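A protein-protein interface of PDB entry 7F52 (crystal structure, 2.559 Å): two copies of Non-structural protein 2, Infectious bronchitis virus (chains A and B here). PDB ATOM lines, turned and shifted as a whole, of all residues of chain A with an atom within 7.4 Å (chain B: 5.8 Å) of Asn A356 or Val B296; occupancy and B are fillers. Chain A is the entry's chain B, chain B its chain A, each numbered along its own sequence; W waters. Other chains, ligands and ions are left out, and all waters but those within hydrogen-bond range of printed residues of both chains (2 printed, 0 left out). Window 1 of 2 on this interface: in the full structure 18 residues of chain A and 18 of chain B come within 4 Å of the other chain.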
ATOM      1  N   THR A 303      24.716 -24.457 -23.956  1.00  0.00           N
ATOM      2  CA  THR A 303      25.144 -23.491 -22.941  1.00  0.00           C
ATOM      3  C   THR A 303      25.673 -24.226 -21.723  1.00  0.00           C
ATOM      4  O   THR A 303      24.991 -25.102 -21.176  1.00  0.00           O
ATOM      5  CB  THR A 303      23.977 -22.586 -22.507  1.00  0.00           C
ATOM      6  OG1 THR A 303      23.441 -21.929 -23.656  1.00  0.00           O
ATOM      7  CG2 THR A 303      24.429 -21.541 -21.520  1.00  0.00           C
ATOM      8  N   GLN A 304      26.889 -23.910 -21.303  1.00  0.00           N
ATOM      9  CA  GLN A 304      27.367 -24.442 -20.026  1.00  0.00           C
ATOM     10  C   GLN A 304      26.618 -23.720 -18.910  1.00  0.00           C
ATOM     11  O   GLN A 304      26.455 -22.506 -18.956  1.00  0.00           O
ATOM     12  CB  GLN A 304      28.873 -24.267 -19.884  1.00  0.00           C
ATOM     13  CG  GLN A 304      29.661 -25.058 -20.913  1.00  0.00           C
ATOM     14  CD  GLN A 304      31.145 -25.067 -20.617  1.00  0.00           C
ATOM     15  OE1 GLN A 304      31.714 -24.051 -20.214  1.00  0.00           O
ATOM     16  NE2 GLN A 304      31.781 -26.217 -20.808  1.00  0.00           N
ATOM     17  N   VAL A 305      26.136 -24.480 -17.937  1.00  0.00           N
ATOM     18  CA  VAL A 305      25.281 -23.957 -16.892  1.00  0.00           C
ATOM     19  C   VAL A 305      25.830 -24.316 -15.502  1.00  0.00           C
ATOM     20  O   VAL A 305      26.585 -25.280 -15.364  1.00  0.00           O
ATOM     21  CB  VAL A 305      23.835 -24.487 -17.058  1.00  0.00           C
ATOM     22  CG1 VAL A 305      23.283 -24.064 -18.383  1.00  0.00           C
ATOM     23  CG2 VAL A 305      23.764 -26.006 -16.919  1.00  0.00           C
ATOM     24  N   VAL A 306      25.483 -23.525 -14.483  1.00  0.00           N
ATOM     25  CA  VAL A 306      25.824 -23.879 -13.103  1.00  0.00           C
ATOM     26  C   VAL A 306      24.565 -24.337 -12.367  1.00  0.00           C
ATOM     27  O   VAL A 306      23.542 -23.647 -12.354  1.00  0.00           O
ATOM     28  CB  VAL A 306      26.499 -22.706 -12.344  1.00  0.00           C
ATOM     29  CG1 VAL A 306      26.475 -22.950 -10.842  1.00  0.00           C
ATOM     30  CG2 VAL A 306      27.937 -22.515 -12.822  1.00  0.00           C
ATOM     31  N   VAL A 307      24.632 -25.527 -11.787  1.00  0.00           N
ATOM     32  CA  VAL A 307      23.491 -26.120 -11.112  1.00  0.00           C
ATOM     33  C   VAL A 307      23.557 -25.847  -9.604  1.00  0.00           C
ATOM     34  O   VAL A 307      24.519 -26.224  -8.944  1.00  0.00           O
ATOM     35  CB  VAL A 307      23.427 -27.639 -11.395  1.00  0.00           C
ATOM     36  CG1 VAL A 307      22.191 -28.267 -10.777  1.00  0.00           C
ATOM     37  CG2 VAL A 307      23.425 -27.876 -12.879  1.00  0.00           C
ATOM     38  N   SER A 327      22.264 -19.099 -17.530  1.00  0.00           N
ATOM     39  CA  SER A 327      23.473 -19.869 -17.263  1.00  0.00           C
ATOM     40  C   SER A 327      23.539 -20.376 -15.811  1.00  0.00           C
ATOM     41  O   SER A 327      24.418 -21.172 -15.467  1.00  0.00           O
ATOM     42  CB  SER A 327      24.722 -19.050 -17.626  1.00  0.00           C
ATOM     43  OG  SER A 327      25.036 -18.095 -16.648  1.00  0.00           O
ATOM     44  N   TYR A 340      17.469 -29.687 -16.890  1.00  0.00           N
ATOM     45  CA  TYR A 340      17.818 -28.382 -16.354  1.00  0.00           C
ATOM     46  C   TYR A 340      16.596 -27.478 -16.253  1.00  0.00           C
ATOM     47  O   TYR A 340      15.830 -27.356 -17.213  1.00  0.00           O
ATOM     48  CB  TYR A 340      18.849 -27.743 -17.259  1.00  0.00           C
ATOM     49  CG  TYR A 340      19.375 -26.398 -16.853  1.00  0.00           C
ATOM     50  CD1 TYR A 340      20.174 -26.253 -15.725  1.00  0.00           C
ATOM     51  CD2 TYR A 340      19.152 -25.286 -17.647  1.00  0.00           C
ATOM     52  CE1 TYR A 340      20.704 -25.046 -15.395  1.00  0.00           C
ATOM     53  CE2 TYR A 340      19.685 -24.073 -17.316  1.00  0.00           C
ATOM     54  CZ  TYR A 340      20.459 -23.968 -16.194  1.00  0.00           C
ATOM     55  OH  TYR A 340      20.985 -22.760 -15.885  1.00  0.00           O
ATOM     56  N   LEU A 353      19.491 -31.435 -20.528  1.00  0.00           N
ATOM     57  CA  LEU A 353      20.755 -31.293 -19.830  1.00  0.00           C
ATOM     58  C   LEU A 353      21.681 -32.469 -20.120  1.00  0.00           C
ATOM     59  O   LEU A 353      21.255 -33.633 -20.093  1.00  0.00           O
ATOM     60  CB  LEU A 353      20.515 -31.183 -18.324  1.00  0.00           C
ATOM     61  CG  LEU A 353      21.784 -31.059 -17.465  1.00  0.00           C
ATOM     62  CD1 LEU A 353      22.469 -29.713 -17.681  1.00  0.00           C
ATOM     63  CD2 LEU A 353      21.491 -31.290 -15.980  1.00  0.00           C
ATOM     64  N   SER A 354      22.946 -32.171 -20.400  1.00  0.00           N
ATOM     65  CA  SER A 354      23.954 -33.220 -20.552  1.00  0.00           C
ATOM     66  C   SER A 354      25.137 -32.901 -19.646  1.00  0.00           C
ATOM     67  O   SER A 354      26.072 -32.203 -20.055  1.00  0.00           O
ATOM     68  CB  SER A 354      24.411 -33.328 -22.007  1.00  0.00           C
ATOM     69  OG  SER A 354      25.370 -34.361 -22.187  1.00  0.00           O
ATOM     70  N   GLY A 355      25.103 -33.396 -18.412  1.00  0.00           N
ATOM     71  CA  GLY A 355      26.156 -33.063 -17.469  1.00  0.00           C
ATOM     72  C   GLY A 355      26.016 -31.598 -17.136  1.00  0.00           C
ATOM     73  O   GLY A 355      25.145 -31.223 -16.364  1.00  0.00           O
ATOM     74  N   ASN A 356      26.842 -30.765 -17.752  1.00  0.00           N
ATOM     75  CA  ASN A 356      26.867 -29.345 -17.424  1.00  0.00           C
ATOM     76  C   ASN A 356      26.425 -28.514 -18.592  1.00  0.00           C
ATOM     77  O   ASN A 356      26.617 -27.285 -18.609  1.00  0.00           O
ATOM     78  CB  ASN A 356      28.276 -28.914 -17.007  1.00  0.00           C
ATOM     79  CG  ASN A 356      29.219 -28.743 -18.194  1.00  0.00           C
ATOM     80  OD1 ASN A 356      29.176 -29.509 -19.158  1.00  0.00           O
ATOM     81  ND2 ASN A 356      30.074 -27.726 -18.132  1.00  0.00           N
ATOM     82  N   PHE A 357      25.843 -29.191 -19.572  1.00  0.00           N
ATOM     83  CA  PHE A 357      25.592 -28.584 -20.858  1.00  0.00           C
ATOM     84  C   PHE A 357      24.095 -28.575 -21.170  1.00  0.00           C
ATOM     85  O   PHE A 357      23.477 -29.639 -21.325  1.00  0.00           O
ATOM     86  CB  PHE A 357      26.366 -29.340 -21.930  1.00  0.00           C
ATOM     87  CG  PHE A 357      26.584 -28.584 -23.199  1.00  0.00           C
ATOM     88  CD1 PHE A 357      27.360 -27.440 -23.220  1.00  0.00           C
ATOM     89  CD2 PHE A 357      26.056 -29.055 -24.399  1.00  0.00           C
ATOM     90  CE1 PHE A 357      27.599 -26.758 -24.417  1.00  0.00           C
ATOM     91  CE2 PHE A 357      26.286 -28.386 -25.597  1.00  0.00           C
ATOM     92  CZ  PHE A 357      27.061 -27.238 -25.610  1.00  0.00           C
ATOM     93  N   ALA A 358      23.512 -27.379 -21.251  1.00  0.00           N
ATOM     94  CA  ALA A 358      22.079 -27.244 -21.517  1.00  0.00           C
ATOM     95  C   ALA A 358      21.808 -26.942 -22.983  1.00  0.00           C
ATOM     96  O   ALA A 358      22.371 -26.004 -23.557  1.00  0.00           O
ATOM     97  CB  ALA A 358      21.424 -26.138 -20.607  1.00  0.00           C
ATOM     98  N   ALA B 276      39.632 -26.606 -16.379  1.00  0.00           N
ATOM     99  CA  ALA B 276      38.341 -27.232 -16.183  1.00  0.00           C
ATOM    100  C   ALA B 276      38.330 -28.072 -14.945  1.00  0.00           C
ATOM    101  O   ALA B 276      39.320 -28.710 -14.616  1.00  0.00           O
ATOM    102  CB  ALA B 276      37.965 -28.076 -17.377  1.00  0.00           C
ATOM    103  N   ALA B 277      37.208 -28.020 -14.238  1.00  0.00           N
ATOM    104  CA  ALA B 277      36.953 -28.893 -13.115  1.00  0.00           C
ATOM    105  C   ALA B 277      36.150 -30.056 -13.635  1.00  0.00           C
ATOM    106  O   ALA B 277      35.264 -29.883 -14.485  1.00  0.00           O
ATOM    107  CB  ALA B 277      36.189 -28.175 -12.040  1.00  0.00           C
ATOM    108  N   VAL B 278      36.428 -31.248 -13.138  1.00  0.00           N
ATOM    109  CA  VAL B 278      35.617 -32.372 -13.568  1.00  0.00           C
ATOM    110  C   VAL B 278      35.231 -33.130 -12.335  1.00  0.00           C
ATOM    111  O   VAL B 278      35.889 -33.062 -11.296  1.00  0.00           O
ATOM    112  CB  VAL B 278      36.348 -33.334 -14.598  1.00  0.00           C
ATOM    113  CG1 VAL B 278      36.652 -32.620 -15.906  1.00  0.00           C
ATOM    114  CG2 VAL B 278      37.621 -33.909 -14.013  1.00  0.00           C
ATOM    115  N   ARG B 279      34.129 -33.838 -12.465  1.00  0.00           N
ATOM    116  CA  ARG B 279      33.715 -34.804 -11.485  1.00  0.00           C
ATOM    117  C   ARG B 279      34.331 -36.158 -11.887  1.00  0.00           C
ATOM    118  O   ARG B 279      34.398 -36.468 -13.077  1.00  0.00           O
ATOM    119  CB  ARG B 279      32.197 -34.827 -11.441  1.00  0.00           C
ATOM    120  CG  ARG B 279      31.591 -35.907 -10.620  1.00  0.00           C
ATOM    121  CD  ARG B 279      30.067 -35.840 -10.735  1.00  0.00           C
ATOM    122  NE  ARG B 279      29.562 -34.527 -11.161  1.00  0.00           N
ATOM    123  CZ  ARG B 279      28.260 -34.210 -11.198  1.00  0.00           C
ATOM    124  NH1 ARG B 279      27.351 -35.106 -10.822  1.00  0.00           N
ATOM    125  NH2 ARG B 279      27.850 -32.998 -11.583  1.00  0.00           N
ATOM    126  N   PHE B 294      35.432 -39.044 -16.496  1.00  0.00           N
ATOM    127  CA  PHE B 294      35.283 -37.679 -16.057  1.00  0.00           C
ATOM    128  C   PHE B 294      33.979 -37.068 -16.564  1.00  0.00           C
ATOM    129  O   PHE B 294      33.537 -37.352 -17.704  1.00  0.00           O
ATOM    130  CB  PHE B 294      36.458 -36.834 -16.538  1.00  0.00           C
ATOM    131  CG  PHE B 294      37.779 -37.289 -16.020  1.00  0.00           C
ATOM    132  CD1 PHE B 294      37.867 -37.968 -14.817  1.00  0.00           C
ATOM    133  CD2 PHE B 294      38.941 -37.012 -16.712  1.00  0.00           C
ATOM    134  CE1 PHE B 294      39.093 -38.388 -14.329  1.00  0.00           C
ATOM    135  CE2 PHE B 294      40.177 -37.432 -16.219  1.00  0.00           C
ATOM    136  CZ  PHE B 294      40.246 -38.120 -15.032  1.00  0.00           C
ATOM    137  N   GLU B 295      33.382 -36.229 -15.708  1.00  0.00           N
ATOM    138  CA  GLU B 295      32.233 -35.406 -16.058  1.00  0.00           C
ATOM    139  C   GLU B 295      32.459 -33.928 -15.706  1.00  0.00           C
ATOM    140  O   GLU B 295      32.371 -33.523 -14.556  1.00  0.00           O
ATOM    141  CB  GLU B 295      30.981 -35.904 -15.349  1.00  0.00           C
ATOM    142  CG  GLU B 295      29.712 -35.183 -15.800  1.00  0.00           C
ATOM    143  CD  GLU B 295      28.499 -35.568 -14.975  1.00  0.00           C
ATOM    144  OE1 GLU B 295      28.109 -36.761 -14.986  1.00  0.00           O
ATOM    145  OE2 GLU B 295      27.950 -34.670 -14.291  1.00  0.00           O
ATOM    146  N   VAL B 296      32.742 -33.129 -16.716  1.00  0.00           N
ATOM    147  CA  VAL B 296      32.973 -31.702 -16.566  1.00  0.00           C
ATOM    148  C   VAL B 296      31.814 -30.941 -15.834  1.00  0.00           C
ATOM    149  O   VAL B 296      30.621 -31.113 -16.159  1.00  0.00           O
ATOM    150  CB  VAL B 296      33.285 -31.137 -18.007  1.00  0.00           C
ATOM    151  CG1 VAL B 296      32.282 -30.143 -18.497  1.00  0.00           C
ATOM    152  CG2 VAL B 296      34.688 -30.568 -18.072  1.00  0.00           C
ATOM    153  N   VAL B 297      32.155 -30.157 -14.806  1.00  0.00           N
ATOM    154  CA  VAL B 297      31.170 -29.291 -14.092  1.00  0.00           C
ATOM    155  C   VAL B 297      31.454 -27.795 -14.218  1.00  0.00           C
ATOM    156  O   VAL B 297      32.602 -27.372 -14.381  1.00  0.00           O
ATOM    157  CB  VAL B 297      31.106 -29.574 -12.571  1.00  0.00           C
ATOM    158  CG1 VAL B 297      30.774 -31.031 -12.297  1.00  0.00           C
ATOM    159  CG2 VAL B 297      32.444 -29.199 -11.904  1.00  0.00           C
ATOM    160  N   GLY B 298      30.409 -26.987 -14.107  1.00  0.00           N
ATOM    161  CA  GLY B 298      30.558 -25.543 -14.191  1.00  0.00           C
ATOM    162  C   GLY B 298      31.124 -25.078 -15.516  1.00  0.00           C
ATOM    163  O   GLY B 298      30.923 -25.719 -16.542  1.00  0.00           O
ATOM    164  N   ASN B 299      31.835 -23.959 -15.505  1.00  0.00           N
ATOM    165  CA  ASN B 299      32.463 -23.447 -16.718  1.00  0.00           C
ATOM    166  C   ASN B 299      33.810 -24.137 -16.999  1.00  0.00           C
ATOM    167  O   ASN B 299      34.664 -24.227 -16.109  1.00  0.00           O
ATOM    168  CB  ASN B 299      32.646 -21.937 -16.597  1.00  0.00           C
ATOM    169  CG  ASN B 299      31.309 -21.196 -16.464  1.00  0.00           C
ATOM    170  OD1 ASN B 299      30.425 -21.365 -17.305  1.00  0.00           O
ATOM    171  ND2 ASN B 299      31.159 -20.373 -15.399  1.00  0.00           N
ATOM    172  N   ALA B 300      33.996 -24.611 -18.232  1.00  0.00           N
ATOM    173  CA  ALA B 300      35.147 -25.457 -18.587  1.00  0.00           C
ATOM    174  C   ALA B 300      35.614 -25.204 -20.014  1.00  0.00           C
ATOM    175  O   ALA B 300      34.809 -25.286 -20.940  1.00  0.00           O
ATOM    176  CB  ALA B 300      34.790 -26.924 -18.421  1.00  0.00           C
ATOM    177  N   SER B 354      35.600 -35.994 -21.349  1.00  0.00           N
ATOM    178  CA  SER B 354      34.315 -35.985 -20.625  1.00  0.00           C
ATOM    179  C   SER B 354      33.215 -36.019 -21.696  1.00  0.00           C
ATOM    180  O   SER B 354      32.919 -34.990 -22.317  1.00  0.00           O
ATOM    181  CB  SER B 354      34.204 -34.747 -19.701  1.00  0.00           C
ATOM    182  OG  SER B 354      32.891 -34.495 -19.206  1.00  0.00           O
ATOM    183  N   PHE B 357      33.848 -34.002 -24.855  1.00  0.00           N
ATOM    184  CA  PHE B 357      34.623 -32.811 -24.556  1.00  0.00           C
ATOM    185  C   PHE B 357      36.060 -33.178 -24.098  1.00  0.00           C
ATOM    186  O   PHE B 357      36.249 -33.860 -23.077  1.00  0.00           O
ATOM    187  CB  PHE B 357      33.896 -31.995 -23.475  1.00  0.00           C
ATOM    188  CG  PHE B 357      34.250 -30.530 -23.452  1.00  0.00           C
ATOM    189  CD1 PHE B 357      34.044 -29.733 -24.564  1.00  0.00           C
ATOM    190  CD2 PHE B 357      34.761 -29.945 -22.296  1.00  0.00           C
ATOM    191  CE1 PHE B 357      34.366 -28.376 -24.534  1.00  0.00           C
ATOM    192  CE2 PHE B 357      35.071 -28.582 -22.241  1.00  0.00           C
ATOM    193  CZ  PHE B 357      34.871 -27.792 -23.354  1.00  0.00           C
ATOM    194  N   LEU B 359      39.775 -32.105 -22.694  1.00  0.00           N
ATOM    195  CA  LEU B 359      40.474 -31.007 -21.998  1.00  0.00           C
ATOM    196  C   LEU B 359      41.875 -30.871 -22.560  1.00  0.00           C
ATOM    197  O   LEU B 359      42.403 -31.808 -23.156  1.00  0.00           O
ATOM    198  CB  LEU B 359      40.525 -31.229 -20.488  1.00  0.00           C
ATOM    199  CG  LEU B 359      39.140 -31.427 -19.849  1.00  0.00           C
ATOM    200  CD1 LEU B 359      39.227 -31.615 -18.320  1.00  0.00           C
ATOM    201  CD2 LEU B 359      38.195 -30.288 -20.207  1.00  0.00           C
HETATM  202  O   HOH W   1      29.334 -32.341 -18.276  1.00  0.00           O
HETATM  203  O   HOH W   2      30.996 -21.709 -19.761  1.00  0.00           O
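The backbone NH of Ala B300 lies within hydrogen-bond range of the side-chain amide oxygen of Gln A304 (3.1 Å).
The backbone carbonyl oxygen (O) of Gly B298 is in hydrogen-bond range of the side-chain amide nitrogen (ND2) of Asn A356, at 2.7 Å.
The backbone NH (N) of Val B296 sits at hydrogen-bond distance from the side-chain hydroxyl (OG) of Ser B354, at 2.8 Å.
The guanidinium group (NH2) of Arg B279 lies within salt-bridge range of the side-chain carboxylate (OE2) of Glu B295, 3.2 Å away.
The backbone carbonyl oxygen (O) of Asn A356 sits at hydrogen-bond distance from the backbone NH (N) of Val A305, 2.9 Å away.
Among the printed residues, pairs that only touch across the chains: Asn A356 with Val B296 (3.2 Å), Gln A304 with Asn B299 (3.6 Å) and Gly A355 with Glu B295 (3.99 Å).
Printed residues of chain B within 4 Å of Gln A304: Asn B299 and Ala B300.
Of the printed residues of chain B, Gly A355 touches Glu B295 (3.99 Å).
Asn A356 touches two residues of chain B.
Ala B276 touches none of the printed residues of chain A.
Of chain A, only Asn A356 (3.2 Å) comes within 4 Å of Val B296.
Printed residues of chain A within 4 Å of Gly B298: Asn A356.
Printed residues of chain A within 4 Å of Ala B300: Gln A304 (3.1 Å).
The nearest residue of chain A that does not touch Val B296 is Gln A304 (4.6 Å).
Of the 13 printed residues of chain A, 3 touch a printed residue of chain B.
Printed residues of chain A that touch a printed residue of chain B: Gln A304, Gly A355 and Asn A356.
Of the 14 printed residues of chain B, 5 touch a printed residue of chain A.
Among the printed residues, no Asp or Glu carboxylate lies within 4 Å of a Lys or Arg side-chain nitrogen of the other chain.
2 positions are printed for both chains.
Of the 5 pairs that touch across the chains among the printed residues, none has its exchanged pair printed and touching as well.
Water W2 bridges the side-chain amide oxygen of Gln A304 (2.5 Å) and the side-chain amide oxygen of Asn B299 (2.5 Å).
Water W1 lies within hydrogen-bond range of the backbone carbonyl oxygen (O) of Val B296 and the side-chain amide oxygen (OD1) of Asn A356.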
